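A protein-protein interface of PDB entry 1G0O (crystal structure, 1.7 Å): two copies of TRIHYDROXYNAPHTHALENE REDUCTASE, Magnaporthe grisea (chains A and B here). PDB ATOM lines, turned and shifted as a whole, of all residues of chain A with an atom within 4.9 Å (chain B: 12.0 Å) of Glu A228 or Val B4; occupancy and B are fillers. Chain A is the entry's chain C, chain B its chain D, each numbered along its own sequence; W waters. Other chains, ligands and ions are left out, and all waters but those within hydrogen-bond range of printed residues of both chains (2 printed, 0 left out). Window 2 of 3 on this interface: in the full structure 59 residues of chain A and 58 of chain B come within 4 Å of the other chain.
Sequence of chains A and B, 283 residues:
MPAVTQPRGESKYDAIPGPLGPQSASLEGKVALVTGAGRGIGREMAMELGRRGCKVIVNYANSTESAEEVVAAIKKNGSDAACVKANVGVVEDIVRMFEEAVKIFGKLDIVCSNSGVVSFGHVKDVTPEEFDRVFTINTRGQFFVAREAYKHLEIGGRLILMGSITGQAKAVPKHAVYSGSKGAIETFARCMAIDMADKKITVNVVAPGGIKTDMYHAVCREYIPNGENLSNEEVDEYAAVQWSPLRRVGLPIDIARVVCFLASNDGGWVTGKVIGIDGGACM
Hydrophobic or aromatic side chains of chain B within 4 Å of the printed part of chain A: Val B4.
Among the printed residues, 6 pairs touch across the chains.
Among the printed residues, no Asp or Glu carboxylate lies within 4 Å of a Lys or Arg side-chain nitrogen of the other chain.
Glu A228 touches just one residue of chain B: Val B4 (3.9 Å).
Arg A221 touches one residue of chain B.
No residue of chain B comes within 4 Å of Gly A227.
No residue of chain B comes within 4 Å of Asn A229.
No residue of chain B comes within 4 Å of Ser A231.
Asn A232 touches just these residues of chain B: Val B4 (3.9 Å), Gln B6 (3.1 Å) and Pro B7 (3.5 Å).
Printed residues of chain A within 4 Å of Gln B6: Asn A232.
Of the printed residues of chain A, Pro B7 touches Asn A232.
Thr B5 touches none of the printed residues of chain A.
The nearest residue of chain B that does not touch Glu A228 is Ala B3 (5.5 Å).
The nearest printed residue of chain A that does not touch Val B4 is Ser A231 (4.4 Å).
The nearest printed residue of chain A that does not touch Pro B7 is Arg A221 (8.5 Å).
No position is printed for both chains.
Of the 6 pairs that touch across the chains among the printed residues, none has its exchanged pair printed and touching as well.
The side-chain amide nitrogen of Asn A232 sits at hydrogen-bond distance from the backbone carbonyl oxygen of Gln B6.
NH2 of Arg A221 sits at hydrogen-bond distance from O of Leu A230 (2.8 Å).
NH2 of Arg A221 sits at hydrogen-bond distance from OD1 of Asn A232.
Among the printed residues, pairs that only touch across the chains: Arg A221 with Val B4, Glu A228 with Val B4, Leu A230 with Val B4, Asn A232 with Val B4 and Asn A232 with Pro B7.
Water W2 bridges the backbone carbonyl oxygen of Val B4 (2.9 Å) and the side-chain amide oxygen of Asn A232 (2.9 Å).
Water W1 bridges the side-chain amide oxygen (OE1) of Gln B6 (2.9 Å) and the backbone NH (N) of Asn A232 (2.9 Å).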
ATOM      1  N   ARG A 221       3.848 -25.099 -31.494  1.00  0.00           N
ATOM      2  CA  ARG A 221       3.302 -24.992 -30.140  1.00  0.00           C
ATOM      3  C   ARG A 221       1.947 -25.686 -29.976  1.00  0.00           C
ATOM      4  O   ARG A 221       1.581 -26.087 -28.879  1.00  0.00           O
ATOM      5  CB  ARG A 221       3.206 -23.518 -29.707  1.00  0.00           C
ATOM      6  CG  ARG A 221       4.554 -22.868 -29.477  1.00  0.00           C
ATOM      7  CD  ARG A 221       4.436 -21.370 -29.280  1.00  0.00           C
ATOM      8  NE  ARG A 221       5.751 -20.754 -29.114  1.00  0.00           N
ATOM      9  CZ  ARG A 221       6.607 -20.515 -30.108  1.00  0.00           C
ATOM     10  NH1 ARG A 221       6.302 -20.833 -31.365  1.00  0.00           N
ATOM     11  NH2 ARG A 221       7.787 -19.973 -29.850  1.00  0.00           N
ATOM     12  N   ASN A 226       0.415 -26.978 -23.277  1.00  0.00           N
ATOM     13  CA  ASN A 226       0.848 -25.782 -22.548  1.00  0.00           C
ATOM     14  C   ASN A 226       2.095 -25.150 -23.165  1.00  0.00           C
ATOM     15  O   ASN A 226       2.950 -24.605 -22.454  1.00  0.00           O
ATOM     16  CB  ASN A 226       1.115 -26.146 -21.081  1.00  0.00           C
ATOM     17  CG  ASN A 226      -0.067 -26.848 -20.439  1.00  0.00           C
ATOM     18  OD1 ASN A 226      -1.186 -26.312 -20.421  1.00  0.00           O
ATOM     19  ND2 ASN A 226       0.152 -28.072 -19.961  1.00  0.00           N
ATOM     20  N   GLY A 227       2.186 -25.211 -24.488  1.00  0.00           N
ATOM     21  CA  GLY A 227       3.346 -24.668 -25.160  1.00  0.00           C
ATOM     22  C   GLY A 227       3.207 -23.261 -25.704  1.00  0.00           C
ATOM     23  O   GLY A 227       4.172 -22.727 -26.250  1.00  0.00           O
ATOM     24  N   GLU A 228       2.042 -22.642 -25.509  1.00  0.00           N
ATOM     25  CA  GLU A 228       1.776 -21.296 -26.026  1.00  0.00           C
ATOM     26  C   GLU A 228       2.829 -20.227 -25.731  1.00  0.00           C
ATOM     27  O   GLU A 228       3.160 -19.424 -26.607  1.00  0.00           O
ATOM     28  CB  GLU A 228       0.393 -20.802 -25.576  1.00  0.00           C
ATOM     29  CG  GLU A 228       0.128 -20.904 -24.066  1.00  0.00           C
ATOM     30  CD  GLU A 228      -0.513 -22.234 -23.620  1.00  0.00           C
ATOM     31  OE1 GLU A 228      -0.903 -23.059 -24.485  1.00  0.00           O
ATOM     32  OE2 GLU A 228      -0.646 -22.441 -22.387  1.00  0.00           O
ATOM     33  N   ASN A 229       3.374 -20.239 -24.517  1.00  0.00           N
ATOM     34  CA  ASN A 229       4.368 -19.254 -24.130  1.00  0.00           C
ATOM     35  C   ASN A 229       5.823 -19.675 -24.202  1.00  0.00           C
ATOM     36  O   ASN A 229       6.702 -18.966 -23.696  1.00  0.00           O
ATOM     37  CB  ASN A 229       4.050 -18.696 -22.750  1.00  0.00           C
ATOM     38  CG  ASN A 229       2.810 -17.855 -22.756  1.00  0.00           C
ATOM     39  OD1 ASN A 229       2.764 -16.800 -23.395  1.00  0.00           O
ATOM     40  ND2 ASN A 229       1.772 -18.340 -22.094  1.00  0.00           N
ATOM     41  N   LEU A 230       6.100 -20.810 -24.835  1.00  0.00           N
ATOM     42  CA  LEU A 230       7.483 -21.246 -24.963  1.00  0.00           C
ATOM     43  C   LEU A 230       8.217 -20.383 -25.998  1.00  0.00           C
ATOM     44  O   LEU A 230       7.642 -20.010 -27.021  1.00  0.00           O
ATOM     45  CB  LEU A 230       7.555 -22.719 -25.378  1.00  0.00           C
ATOM     46  CG  LEU A 230       7.001 -23.760 -24.413  1.00  0.00           C
ATOM     47  CD1 LEU A 230       7.091 -25.142 -25.057  1.00  0.00           C
ATOM     48  CD2 LEU A 230       7.783 -23.719 -23.125  1.00  0.00           C
ATOM     49  N   SER A 231       9.475 -20.052 -25.717  1.00  0.00           N
ATOM     50  CA  SER A 231      10.299 -19.263 -26.635  1.00  0.00           C
ATOM     51  C   SER A 231      10.647 -20.156 -27.821  1.00  0.00           C
ATOM     52  O   SER A 231      10.498 -21.380 -27.740  1.00  0.00           O
ATOM     53  CB  SER A 231      11.612 -18.854 -25.955  1.00  0.00           C
ATOM     54  OG  SER A 231      12.458 -19.982 -25.748  1.00  0.00           O
ATOM     55  N   ASN A 232      11.177 -19.559 -28.891  1.00  0.00           N
ATOM     56  CA  ASN A 232      11.559 -20.330 -30.080  1.00  0.00           C
ATOM     57  C   ASN A 232      12.607 -21.379 -29.691  1.00  0.00           C
ATOM     58  O   ASN A 232      12.544 -22.517 -30.137  1.00  0.00           O
ATOM     59  CB  ASN A 232      12.089 -19.413 -31.199  1.00  0.00           C
ATOM     60  CG  ASN A 232      10.991 -18.547 -31.840  1.00  0.00           C
ATOM     61  OD1 ASN A 232       9.799 -18.774 -31.644  1.00  0.00           O
ATOM     62  ND2 ASN A 232      11.401 -17.557 -32.613  1.00  0.00           N
ATOM     63  N   ALA B   3       1.778 -14.087 -27.088  1.00  0.00           N
ATOM     64  CA  ALA B   3       2.289 -14.301 -28.444  1.00  0.00           C
ATOM     65  C   ALA B   3       3.807 -14.143 -28.510  1.00  0.00           C
ATOM     66  O   ALA B   3       4.358 -13.177 -27.984  1.00  0.00           O
ATOM     67  CB  ALA B   3       1.620 -13.346 -29.430  1.00  0.00           C
ATOM     68  N   VAL B   4       4.477 -15.120 -29.121  1.00  0.00           N
ATOM     69  CA  VAL B   4       5.929 -15.104 -29.278  1.00  0.00           C
ATOM     70  C   VAL B   4       6.129 -14.647 -30.720  1.00  0.00           C
ATOM     71  O   VAL B   4       5.966 -15.425 -31.672  1.00  0.00           O
ATOM     72  CB  VAL B   4       6.534 -16.505 -29.044  1.00  0.00           C
ATOM     73  CG1 VAL B   4       8.065 -16.439 -29.080  1.00  0.00           C
ATOM     74  CG2 VAL B   4       6.051 -17.055 -27.698  1.00  0.00           C
ATOM     75  N   THR B   5       6.444 -13.366 -30.871  1.00  0.00           N
ATOM     76  CA  THR B   5       6.579 -12.751 -32.185  1.00  0.00           C
ATOM     77  C   THR B   5       7.929 -12.854 -32.898  1.00  0.00           C
ATOM     78  O   THR B   5       8.027 -12.492 -34.077  1.00  0.00           O
ATOM     79  CB  THR B   5       6.154 -11.266 -32.124  1.00  0.00           C
ATOM     80  OG1 THR B   5       7.107 -10.539 -31.353  1.00  0.00           O
ATOM     81  CG2 THR B   5       4.763 -11.121 -31.460  1.00  0.00           C
ATOM     82  N   GLN B   6       8.969 -13.309 -32.195  1.00  0.00           N
ATOM     83  CA  GLN B   6      10.298 -13.442 -32.809  1.00  0.00           C
ATOM     84  C   GLN B   6      10.233 -14.299 -34.064  1.00  0.00           C
ATOM     85  O   GLN B   6       9.675 -15.395 -34.051  1.00  0.00           O
ATOM     86  CB  GLN B   6      11.317 -14.080 -31.856  1.00  0.00           C
ATOM     87  CG  GLN B   6      11.891 -13.155 -30.777  1.00  0.00           C
ATOM     88  CD  GLN B   6      11.096 -13.203 -29.486  1.00  0.00           C
ATOM     89  OE1 GLN B   6      10.174 -14.020 -29.342  1.00  0.00           O
ATOM     90  NE2 GLN B   6      11.451 -12.339 -28.534  1.00  0.00           N
ATOM     91  N   PRO B   7      10.771 -13.791 -35.178  1.00  0.00           N
ATOM     92  CA  PRO B   7      10.753 -14.560 -36.427  1.00  0.00           C
ATOM     93  C   PRO B   7      11.702 -15.758 -36.286  1.00  0.00           C
ATOM     94  O   PRO B   7      12.568 -15.767 -35.409  1.00  0.00           O
ATOM     95  CB  PRO B   7      11.301 -13.559 -37.455  1.00  0.00           C
ATOM     96  CG  PRO B   7      11.073 -12.206 -36.816  1.00  0.00           C
ATOM     97  CD  PRO B   7      11.377 -12.464 -35.379  1.00  0.00           C
ATOM     98  N   ARG B   8      11.548 -16.750 -37.161  1.00  0.00           N
ATOM     99  CA  ARG B   8      12.400 -17.940 -37.147  1.00  0.00           C
ATOM    100  C   ARG B   8      13.841 -17.511 -37.106  1.00  0.00           C
ATOM    101  O   ARG B   8      14.202 -16.459 -37.638  1.00  0.00           O
ATOM    102  CB  ARG B   8      12.196 -18.792 -38.408  1.00  0.00           C
ATOM    103  CG  ARG B   8      11.548 -20.140 -38.138  1.00  0.00           C
ATOM    104  CD  ARG B   8      11.974 -21.234 -39.118  1.00  0.00           C
ATOM    105  NE  ARG B   8      11.547 -20.982 -40.497  1.00  0.00           N
ATOM    106  CZ  ARG B   8      12.234 -21.381 -41.571  1.00  0.00           C
ATOM    107  NH1 ARG B   8      13.384 -22.035 -41.422  1.00  0.00           N
ATOM    108  NH2 ARG B   8      11.745 -21.184 -42.793  1.00  0.00           N
ATOM    109  N   GLY B   9      14.664 -18.320 -36.461  1.00  0.00           N
ATOM    110  CA  GLY B   9      16.068 -17.998 -36.375  1.00  0.00           C
ATOM    111  C   GLY B   9      16.915 -19.251 -36.447  1.00  0.00           C
ATOM    112  O   GLY B   9      16.460 -20.369 -36.136  1.00  0.00           O
HETATM  113  O   HOH W   1      11.473 -16.628 -28.974  1.00  0.00           O
HETATM  114  O   HOH W   2       7.357 -17.687 -32.711  1.00  0.00           O
